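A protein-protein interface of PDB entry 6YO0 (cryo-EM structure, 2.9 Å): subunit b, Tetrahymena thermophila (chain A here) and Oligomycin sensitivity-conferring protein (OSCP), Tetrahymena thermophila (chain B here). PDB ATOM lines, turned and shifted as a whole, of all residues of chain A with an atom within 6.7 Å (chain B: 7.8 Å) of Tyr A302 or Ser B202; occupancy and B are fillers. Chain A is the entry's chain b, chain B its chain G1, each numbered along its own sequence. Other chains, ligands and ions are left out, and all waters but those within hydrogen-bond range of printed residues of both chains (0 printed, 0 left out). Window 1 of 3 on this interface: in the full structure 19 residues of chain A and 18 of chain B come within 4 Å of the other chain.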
ATOM      1  N   SER A 287      13.799 -11.253  -6.761  1.00  0.00           N
ATOM      2  CA  SER A 287      13.193 -12.425  -7.379  1.00  0.00           C
ATOM      3  C   SER A 287      12.204 -13.087  -6.432  1.00  0.00           C
ATOM      4  O   SER A 287      11.116 -13.502  -6.849  1.00  0.00           O
ATOM      5  CB  SER A 287      14.274 -13.413  -7.804  1.00  0.00           C
ATOM      6  OG  SER A 287      15.193 -12.799  -8.690  1.00  0.00           O
ATOM      7  N   SER A 290       9.093 -10.974  -6.491  1.00  0.00           N
ATOM      8  CA  SER A 290       8.384 -11.190  -7.745  1.00  0.00           C
ATOM      9  C   SER A 290       7.840 -12.608  -7.837  1.00  0.00           C
ATOM     10  O   SER A 290       6.758 -12.822  -8.395  1.00  0.00           O
ATOM     11  CB  SER A 290       9.308 -10.899  -8.926  1.00  0.00           C
ATOM     12  OG  SER A 290       8.611 -10.995 -10.154  1.00  0.00           O
ATOM     13  N   ALA A 291       8.568 -13.582  -7.288  1.00  0.00           N
ATOM     14  CA  ALA A 291       8.090 -14.959  -7.312  1.00  0.00           C
ATOM     15  C   ALA A 291       6.856 -15.137  -6.439  1.00  0.00           C
ATOM     16  O   ALA A 291       5.886 -15.777  -6.857  1.00  0.00           O
ATOM     17  CB  ALA A 291       9.202 -15.901  -6.858  1.00  0.00           C
ATOM     18  N   MET A 300       2.912 -15.564 -13.925  1.00  0.00           N
ATOM     19  CA  MET A 300       4.124 -14.904 -13.459  1.00  0.00           C
ATOM     20  C   MET A 300       4.638 -13.966 -14.535  1.00  0.00           C
ATOM     21  O   MET A 300       4.903 -14.396 -15.662  1.00  0.00           O
ATOM     22  CB  MET A 300       5.197 -15.931 -13.098  1.00  0.00           C
ATOM     23  CG  MET A 300       6.573 -15.341 -12.864  1.00  0.00           C
ATOM     24  SD  MET A 300       6.642 -14.112 -11.559  1.00  0.00           S
ATOM     25  CE  MET A 300       8.388 -13.721 -11.616  1.00  0.00           C
ATOM     26  N   ASP A 301       4.782 -12.691 -14.184  1.00  0.00           N
ATOM     27  CA  ASP A 301       5.395 -11.697 -15.052  1.00  0.00           C
ATOM     28  C   ASP A 301       6.489 -10.983 -14.278  1.00  0.00           C
ATOM     29  O   ASP A 301       6.311 -10.637 -13.106  1.00  0.00           O
ATOM     30  CB  ASP A 301       4.370 -10.682 -15.555  1.00  0.00           C
ATOM     31  CG  ASP A 301       3.334 -11.301 -16.463  1.00  0.00           C
ATOM     32  OD1 ASP A 301       3.455 -12.504 -16.764  1.00  0.00           O
ATOM     33  OD2 ASP A 301       2.398 -10.584 -16.873  1.00  0.00           O
ATOM     34  N   TYR A 302       7.619 -10.767 -14.939  1.00  0.00           N
ATOM     35  CA  TYR A 302       8.789 -10.162 -14.308  1.00  0.00           C
ATOM     36  C   TYR A 302       8.760  -8.639 -14.395  1.00  0.00           C
ATOM     37  O   TYR A 302       9.695  -8.007 -14.885  1.00  0.00           O
ATOM     38  CB  TYR A 302      10.054 -10.732 -14.933  1.00  0.00           C
ATOM     39  CG  TYR A 302      10.166 -12.231 -14.781  1.00  0.00           C
ATOM     40  CD1 TYR A 302      11.048 -12.790 -13.871  1.00  0.00           C
ATOM     41  CD2 TYR A 302       9.392 -13.087 -15.548  1.00  0.00           C
ATOM     42  CE1 TYR A 302      11.152 -14.155 -13.727  1.00  0.00           C
ATOM     43  CE2 TYR A 302       9.490 -14.453 -15.410  1.00  0.00           C
ATOM     44  CZ  TYR A 302      10.372 -14.982 -14.499  1.00  0.00           C
ATOM     45  OH  TYR A 302      10.475 -16.343 -14.357  1.00  0.00           O
ATOM     46  N   GLN A 303       7.671  -8.036 -13.916  1.00  0.00           N
ATOM     47  CA  GLN A 303       7.560  -6.581 -13.952  1.00  0.00           C
ATOM     48  C   GLN A 303       8.611  -5.908 -13.081  1.00  0.00           C
ATOM     49  O   GLN A 303       9.009  -4.771 -13.358  1.00  0.00           O
ATOM     50  CB  GLN A 303       6.167  -6.146 -13.503  1.00  0.00           C
ATOM     51  CG  GLN A 303       5.060  -6.489 -14.480  1.00  0.00           C
ATOM     52  CD  GLN A 303       4.278  -7.720 -14.073  1.00  0.00           C
ATOM     53  OE1 GLN A 303       4.717  -8.500 -13.228  1.00  0.00           O
ATOM     54  NE2 GLN A 303       3.107  -7.897 -14.672  1.00  0.00           N
ATOM     55  N   ASN A 304       9.069  -6.584 -12.028  1.00  0.00           N
ATOM     56  CA  ASN A 304       9.959  -5.986 -11.043  1.00  0.00           C
ATOM     57  C   ASN A 304      11.351  -6.605 -11.041  1.00  0.00           C
ATOM     58  O   ASN A 304      12.159  -6.278 -10.166  1.00  0.00           O
ATOM     59  CB  ASN A 304       9.336  -6.097  -9.652  1.00  0.00           C
ATOM     60  CG  ASN A 304       7.900  -5.620  -9.622  1.00  0.00           C
ATOM     61  OD1 ASN A 304       7.491  -4.797 -10.441  1.00  0.00           O
ATOM     62  ND2 ASN A 304       7.124  -6.136  -8.678  1.00  0.00           N
ATOM     63  N   ASP A 305      11.651  -7.486 -11.986  1.00  0.00           N
ATOM     64  CA  ASP A 305      12.964  -8.107 -12.008  1.00  0.00           C
ATOM     65  C   ASP A 305      14.044  -7.051 -12.228  1.00  0.00           C
ATOM     66  O   ASP A 305      13.842  -6.105 -12.999  1.00  0.00           O
ATOM     67  CB  ASP A 305      13.041  -9.162 -13.107  1.00  0.00           C
ATOM     68  CG  ASP A 305      12.941  -8.560 -14.494  1.00  0.00           C
ATOM     69  OD1 ASP A 305      12.346  -7.471 -14.628  1.00  0.00           O
ATOM     70  OD2 ASP A 305      13.459  -9.176 -15.450  1.00  0.00           O
ATOM     71  N   PRO A 306      15.199  -7.176 -11.568  1.00  0.00           N
ATOM     72  CA  PRO A 306      16.258  -6.174 -11.741  1.00  0.00           C
ATOM     73  C   PRO A 306      17.150  -6.423 -12.941  1.00  0.00           C
ATOM     74  O   PRO A 306      17.896  -5.517 -13.337  1.00  0.00           O
ATOM     75  CB  PRO A 306      17.059  -6.298 -10.441  1.00  0.00           C
ATOM     76  CG  PRO A 306      16.929  -7.745 -10.097  1.00  0.00           C
ATOM     77  CD  PRO A 306      15.553  -8.173 -10.544  1.00  0.00           C
ATOM     78  N   LEU A 308      16.478  -6.757 -16.174  1.00  0.00           N
ATOM     79  CA  LEU A 308      16.201  -5.901 -17.323  1.00  0.00           C
ATOM     80  C   LEU A 308      16.640  -4.464 -17.089  1.00  0.00           C
ATOM     81  O   LEU A 308      17.313  -3.897 -17.967  1.00  0.00           O
ATOM     82  CB  LEU A 308      14.710  -5.980 -17.661  1.00  0.00           C
ATOM     83  CG  LEU A 308      14.244  -5.190 -18.880  1.00  0.00           C
ATOM     84  CD1 LEU A 308      15.001  -5.641 -20.114  1.00  0.00           C
ATOM     85  CD2 LEU A 308      12.753  -5.359 -19.075  1.00  0.00           C
ATOM     86  N   ILE B 150      10.423 -25.459  -4.933  1.00  0.00           N
ATOM     87  CA  ILE B 150      11.845 -25.668  -5.172  1.00  0.00           C
ATOM     88  C   ILE B 150      12.526 -24.310  -5.279  1.00  0.00           C
ATOM     89  O   ILE B 150      12.156 -23.486  -6.125  1.00  0.00           O
ATOM     90  CB  ILE B 150      12.087 -26.505  -6.435  1.00  0.00           C
ATOM     91  CG1 ILE B 150      11.199 -27.749  -6.417  1.00  0.00           C
ATOM     92  CG2 ILE B 150      13.549 -26.889  -6.536  1.00  0.00           C
ATOM     93  CD1 ILE B 150      11.241 -28.548  -7.696  1.00  0.00           C
ATOM     94  N   ILE B 186      18.877 -23.638 -10.443  1.00  0.00           N
ATOM     95  CA  ILE B 186      18.351 -22.278 -10.519  1.00  0.00           C
ATOM     96  C   ILE B 186      18.775 -21.499  -9.280  1.00  0.00           C
ATOM     97  O   ILE B 186      19.228 -22.062  -8.278  1.00  0.00           O
ATOM     98  CB  ILE B 186      16.823 -22.258 -10.676  1.00  0.00           C
ATOM     99  CG1 ILE B 186      16.126 -22.759  -9.416  1.00  0.00           C
ATOM    100  CG2 ILE B 186      16.420 -23.137 -11.829  1.00  0.00           C
ATOM    101  CD1 ILE B 186      14.631 -22.711  -9.500  1.00  0.00           C
ATOM    102  N   LEU B 187      18.655 -20.175  -9.367  1.00  0.00           N
ATOM    103  CA  LEU B 187      18.978 -19.295  -8.255  1.00  0.00           C
ATOM    104  C   LEU B 187      17.844 -18.310  -8.027  1.00  0.00           C
ATOM    105  O   LEU B 187      17.236 -17.817  -8.981  1.00  0.00           O
ATOM    106  CB  LEU B 187      20.267 -18.513  -8.518  1.00  0.00           C
ATOM    107  CG  LEU B 187      21.546 -19.301  -8.806  1.00  0.00           C
ATOM    108  CD1 LEU B 187      21.529 -19.851 -10.227  1.00  0.00           C
ATOM    109  CD2 LEU B 187      22.781 -18.441  -8.572  1.00  0.00           C
ATOM    110  N   GLY B 188      17.561 -18.030  -6.755  1.00  0.00           N
ATOM    111  CA  GLY B 188      16.569 -17.037  -6.389  1.00  0.00           C
ATOM    112  C   GLY B 188      15.198 -17.268  -6.985  1.00  0.00           C
ATOM    113  O   GLY B 188      14.343 -16.378  -6.949  1.00  0.00           O
ATOM    114  N   GLY B 189      14.973 -18.455  -7.535  1.00  0.00           N
ATOM    115  CA  GLY B 189      13.733 -18.781  -8.210  1.00  0.00           C
ATOM    116  C   GLY B 189      12.872 -19.744  -7.419  1.00  0.00           C
ATOM    117  O   GLY B 189      13.378 -20.554  -6.638  1.00  0.00           O
ATOM    118  N   LEU B 190      11.561 -19.647  -7.622  1.00  0.00           N
ATOM    119  CA  LEU B 190      10.593 -20.529  -6.987  1.00  0.00           C
ATOM    120  C   LEU B 190       9.845 -21.307  -8.057  1.00  0.00           C
ATOM    121  O   LEU B 190       9.379 -20.726  -9.042  1.00  0.00           O
ATOM    122  CB  LEU B 190       9.593 -19.741  -6.141  1.00  0.00           C
ATOM    123  CG  LEU B 190      10.074 -19.189  -4.804  1.00  0.00           C
ATOM    124  CD1 LEU B 190      10.431 -20.297  -3.833  1.00  0.00           C
ATOM    125  CD2 LEU B 190      11.244 -18.264  -5.022  1.00  0.00           C
ATOM    126  N   GLN B 191       9.736 -22.617  -7.862  1.00  0.00           N
ATOM    127  CA  GLN B 191       8.956 -23.484  -8.734  1.00  0.00           C
ATOM    128  C   GLN B 191       8.003 -24.292  -7.872  1.00  0.00           C
ATOM    129  O   GLN B 191       8.444 -25.022  -6.978  1.00  0.00           O
ATOM    130  CB  GLN B 191       9.860 -24.399  -9.559  1.00  0.00           C
ATOM    131  CG  GLN B 191      10.871 -23.647 -10.399  1.00  0.00           C
ATOM    132  CD  GLN B 191      11.731 -24.547 -11.271  1.00  0.00           C
ATOM    133  OE1 GLN B 191      12.724 -24.098 -11.839  1.00  0.00           O
ATOM    134  NE2 GLN B 191      11.355 -25.816 -11.386  1.00  0.00           N
ATOM    135  N   MET B 192       6.709 -24.164  -8.136  1.00  0.00           N
ATOM    136  CA  MET B 192       5.675 -24.828  -7.358  1.00  0.00           C
ATOM    137  C   MET B 192       5.093 -25.987  -8.153  1.00  0.00           C
ATOM    138  O   MET B 192       4.718 -25.826  -9.318  1.00  0.00           O
ATOM    139  CB  MET B 192       4.578 -23.843  -6.947  1.00  0.00           C
ATOM    140  CG  MET B 192       3.697 -23.342  -8.074  1.00  0.00           C
ATOM    141  SD  MET B 192       2.125 -22.662  -7.523  1.00  0.00           S
ATOM    142  CE  MET B 192       1.390 -24.112  -6.789  1.00  0.00           C
ATOM    143  N   PHE B 198       2.418 -27.219 -12.772  1.00  0.00           N
ATOM    144  CA  PHE B 198       3.759 -26.702 -12.552  1.00  0.00           C
ATOM    145  C   PHE B 198       3.799 -25.243 -12.966  1.00  0.00           C
ATOM    146  O   PHE B 198       3.383 -24.897 -14.076  1.00  0.00           O
ATOM    147  CB  PHE B 198       4.781 -27.512 -13.340  1.00  0.00           C
ATOM    148  CG  PHE B 198       6.135 -26.884 -13.416  1.00  0.00           C
ATOM    149  CD1 PHE B 198       6.998 -26.951 -12.343  1.00  0.00           C
ATOM    150  CD2 PHE B 198       6.553 -26.247 -14.564  1.00  0.00           C
ATOM    151  CE1 PHE B 198       8.250 -26.385 -12.408  1.00  0.00           C
ATOM    152  CE2 PHE B 198       7.803 -25.679 -14.635  1.00  0.00           C
ATOM    153  CZ  PHE B 198       8.653 -25.749 -13.555  1.00  0.00           C
ATOM    154  N   LEU B 199       4.299 -24.393 -12.076  1.00  0.00           N
ATOM    155  CA  LEU B 199       4.401 -22.961 -12.317  1.00  0.00           C
ATOM    156  C   LEU B 199       5.824 -22.522 -12.028  1.00  0.00           C
ATOM    157  O   LEU B 199       6.299 -22.652 -10.896  1.00  0.00           O
ATOM    158  CB  LEU B 199       3.404 -22.190 -11.450  1.00  0.00           C
ATOM    159  CG  LEU B 199       3.101 -20.736 -11.796  1.00  0.00           C
ATOM    160  CD1 LEU B 199       4.315 -19.890 -11.553  1.00  0.00           C
ATOM    161  CD2 LEU B 199       2.662 -20.601 -13.231  1.00  0.00           C
ATOM    162  N   ASP B 200       6.501 -22.009 -13.050  1.00  0.00           N
ATOM    163  CA  ASP B 200       7.906 -21.645 -12.956  1.00  0.00           C
ATOM    164  C   ASP B 200       8.043 -20.134 -12.856  1.00  0.00           C
ATOM    165  O   ASP B 200       7.710 -19.409 -13.800  1.00  0.00           O
ATOM    166  CB  ASP B 200       8.684 -22.162 -14.164  1.00  0.00           C
ATOM    167  CG  ASP B 200      10.104 -21.643 -14.201  1.00  0.00           C
ATOM    168  OD1 ASP B 200      10.803 -21.749 -13.173  1.00  0.00           O
ATOM    169  OD2 ASP B 200      10.522 -21.135 -15.261  1.00  0.00           O
ATOM    170  N   CYS B 201       8.543 -19.668 -11.714  1.00  0.00           N
ATOM    171  CA  CYS B 201       8.902 -18.274 -11.503  1.00  0.00           C
ATOM    172  C   CYS B 201      10.408 -18.123 -11.364  1.00  0.00           C
ATOM    173  O   CYS B 201      10.889 -17.100 -10.869  1.00  0.00           O
ATOM    174  CB  CYS B 201       8.199 -17.719 -10.268  1.00  0.00           C
ATOM    175  SG  CYS B 201       6.407 -17.859 -10.310  1.00  0.00           S
ATOM    176  N   SER B 202      11.156 -19.132 -11.794  1.00  0.00           N
ATOM    177  CA  SER B 202      12.592 -19.144 -11.586  1.00  0.00           C
ATOM    178  C   SER B 202      13.276 -18.025 -12.352  1.00  0.00           C
ATOM    179  O   SER B 202      12.919 -17.716 -13.492  1.00  0.00           O
ATOM    180  CB  SER B 202      13.176 -20.486 -12.013  1.00  0.00           C
ATOM    181  OG  SER B 202      12.859 -20.763 -13.363  1.00  0.00           O
ATOM    182  N   LEU B 203      14.272 -17.422 -11.709  1.00  0.00           N
ATOM    183  CA  LEU B 203      15.118 -16.453 -12.384  1.00  0.00           C
ATOM    184  C   LEU B 203      15.951 -17.097 -13.478  1.00  0.00           C
ATOM    185  O   LEU B 203      16.346 -16.412 -14.428  1.00  0.00           O
ATOM    186  CB  LEU B 203      16.017 -15.768 -11.358  1.00  0.00           C
ATOM    187  CG  LEU B 203      17.224 -14.985 -11.865  1.00  0.00           C
ATOM    188  CD1 LEU B 203      17.553 -13.894 -10.874  1.00  0.00           C
ATOM    189  CD2 LEU B 203      18.428 -15.888 -12.077  1.00  0.00           C
ATOM    190  N   LEU B 204      16.218 -18.399 -13.371  1.00  0.00           N
ATOM    191  CA  LEU B 204      16.963 -19.088 -14.418  1.00  0.00           C
ATOM    192  C   LEU B 204      16.230 -18.991 -15.747  1.00  0.00           C
ATOM    193  O   LEU B 204      16.853 -18.819 -16.801  1.00  0.00           O
ATOM    194  CB  LEU B 204      17.182 -20.546 -14.016  1.00  0.00           C
ATOM    195  CG  LEU B 204      17.863 -21.505 -14.995  1.00  0.00           C
ATOM    196  CD1 LEU B 204      16.897 -22.053 -16.028  1.00  0.00           C
ATOM    197  CD2 LEU B 204      19.037 -20.824 -15.664  1.00  0.00           C
ATOM    198  N   SER B 205      14.902 -19.087 -15.714  1.00  0.00           N
ATOM    199  CA  SER B 205      14.120 -18.952 -16.936  1.00  0.00           C
ATOM    200  C   SER B 205      14.269 -17.556 -17.516  1.00  0.00           C
ATOM    201  O   SER B 205      14.412 -17.388 -18.732  1.00  0.00           O
ATOM    202  CB  SER B 205      12.653 -19.253 -16.651  1.00  0.00           C
ATOM    203  OG  SER B 205      11.860 -19.054 -17.805  1.00  0.00           O
ATOM    204  N   ARG B 206      14.240 -16.543 -16.654  1.00  0.00           N
ATOM    205  CA  ARG B 206      14.423 -15.173 -17.109  1.00  0.00           C
ATOM    206  C   ARG B 206      15.789 -14.994 -17.757  1.00  0.00           C
ATOM    207  O   ARG B 206      15.913 -14.335 -18.795  1.00  0.00           O
ATOM    208  CB  ARG B 206      14.246 -14.220 -15.928  1.00  0.00           C
ATOM    209  CG  ARG B 206      14.351 -12.747 -16.256  1.00  0.00           C
ATOM    210  CD  ARG B 206      13.168 -12.277 -17.066  1.00  0.00           C
ATOM    211  NE  ARG B 206      13.114 -10.827 -17.182  1.00  0.00           N
ATOM    212  CZ  ARG B 206      12.139 -10.168 -17.798  1.00  0.00           C
ATOM    213  NH1 ARG B 206      12.167  -8.847 -17.853  1.00  0.00           N
ATOM    214  NH2 ARG B 206      11.143 -10.831 -18.364  1.00  0.00           N
ATOM    215  N   VAL B 207      16.826 -15.585 -17.166  1.00  0.00           N
ATOM    216  CA  VAL B 207      18.164 -15.477 -17.737  1.00  0.00           C
ATOM    217  C   VAL B 207      18.200 -16.074 -19.136  1.00  0.00           C
ATOM    218  O   VAL B 207      18.687 -15.451 -20.087  1.00  0.00           O
ATOM    219  CB  VAL B 207      19.186 -16.162 -16.818  1.00  0.00           C
ATOM    220  CG1 VAL B 207      20.531 -16.240 -17.498  1.00  0.00           C
ATOM    221  CG2 VAL B 207      19.289 -15.420 -15.508  1.00  0.00           C
ATOM    222  N   ASN B 208      17.678 -17.290 -19.286  1.00  0.00           N
ATOM    223  CA  ASN B 208      17.693 -17.943 -20.589  1.00  0.00           C
ATOM    224  C   ASN B 208      16.869 -17.171 -21.609  1.00  0.00           C
ATOM    225  O   ASN B 208      17.297 -16.985 -22.753  1.00  0.00           O
ATOM    226  CB  ASN B 208      17.181 -19.373 -20.458  1.00  0.00           C
ATOM    227  CG  ASN B 208      18.102 -20.243 -19.633  1.00  0.00           C
ATOM    228  OD1 ASN B 208      19.283 -19.935 -19.471  1.00  0.00           O
ATOM    229  ND2 ASN B 208      17.569 -21.337 -19.107  1.00  0.00           N
ATOM    230  N   LYS B 209      15.685 -16.708 -21.211  1.00  0.00           N
ATOM    231  CA  LYS B 209      14.825 -15.983 -22.139  1.00  0.00           C
ATOM    232  C   LYS B 209      15.515 -14.734 -22.671  1.00  0.00           C
ATOM    233  O   LYS B 209      15.475 -14.459 -23.875  1.00  0.00           O
ATOM    234  CB  LYS B 209      13.512 -15.621 -21.449  1.00  0.00           C
ATOM    235  CG  LYS B 209      12.510 -14.883 -22.316  1.00  0.00           C
ATOM    236  CD  LYS B 209      12.027 -15.750 -23.466  1.00  0.00           C
ATOM    237  CE  LYS B 209      11.107 -14.992 -24.414  1.00  0.00           C
ATOM    238  NZ  LYS B 209       9.908 -14.419 -23.743  1.00  0.00           N
ATOM    239  N   LEU B 210      16.160 -13.969 -21.792  1.00  0.00           N
ATOM    240  CA  LEU B 210      16.829 -12.749 -22.228  1.00  0.00           C
ATOM    241  C   LEU B 210      17.995 -13.051 -23.159  1.00  0.00           C
ATOM    242  O   LEU B 210      18.146 -12.408 -24.204  1.00  0.00           O
ATOM    243  CB  LEU B 210      17.304 -11.952 -21.017  1.00  0.00           C
ATOM    244  CG  LEU B 210      16.301 -10.983 -20.394  1.00  0.00           C
ATOM    245  CD1 LEU B 210      15.012 -11.661 -19.989  1.00  0.00           C
ATOM    246  CD2 LEU B 210      16.940 -10.310 -19.199  1.00  0.00           C
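Among the printed residues, pairs that only touch across the chains: Ser A287 with Gly B188 (3.1 Å), Ser A287 with Leu B203 (3.4 Å), Ala A291 with Leu B190 (3.6 Å), Ala A291 with Cys B201 (3.99 Å), Met A300 with Cys B201 (3.6 Å), Tyr A302 with Cys B201 (3.5 Å), Tyr A302 with Arg B206 (3.6 Å) and Leu A308 with Arg B206 (3.7 Å).
Hydrophobic or aromatic side chains of chain B within 4 Å of the printed part of chain A: Leu B190 and Leu B203.
Printed residues of chain A that touch a printed residue of chain B: Ser A287, Ala A291, Met A300, Tyr A302, Asp A305 and Leu A308.
Hydrophobic or aromatic side chains of chain A within 4 Å of the printed part of chain B: Ala A291, Met A300, Tyr A302 and Leu A308.
Tyr A302 touches three residues of chain B.
Of the printed residues of chain A, Ser B202 touches Tyr A302 (2.9 Å).
Printed residues of chain A within 4 Å of Leu B190: Ala A291 (3.6 Å).
Printed residues of chain B within 4 Å of Leu A308: Arg B206.
Printed residues of chain B within 4 Å of Ser A287: Gly B188 (3.1 Å) and Leu B203 (3.4 Å).
Printed residues of chain A within 4 Å of Arg B206: Tyr A302, Asp A305 and Leu A308.
The nearest residue of chain B that does not touch Tyr A302 is Asp B200 (4.2 Å).
The nearest printed residue of chain B that does not touch Ala A291 is Gly B188 (5.2 Å).
O of Leu B190 sits at hydrogen-bond distance from N of Cys B201, 3.0 Å away.
The backbone NH (N) of Ser B202 sits close to the side-chain carboxylate (OD1) of Asp B200 (3.0 Å).
OD1 of Asp A305 lies close to O of Tyr A302 (2.7 Å).
The backbone carbonyl oxygen of Ser B202 sits at hydrogen-bond distance from the side-chain hydroxyl of Tyr A302, 2.9 Å away.
The side-chain carboxylate (OD2) of Asp A305 lies within salt-bridge range of the guanidinium group (NE) of Arg B206 (2.4 Å).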
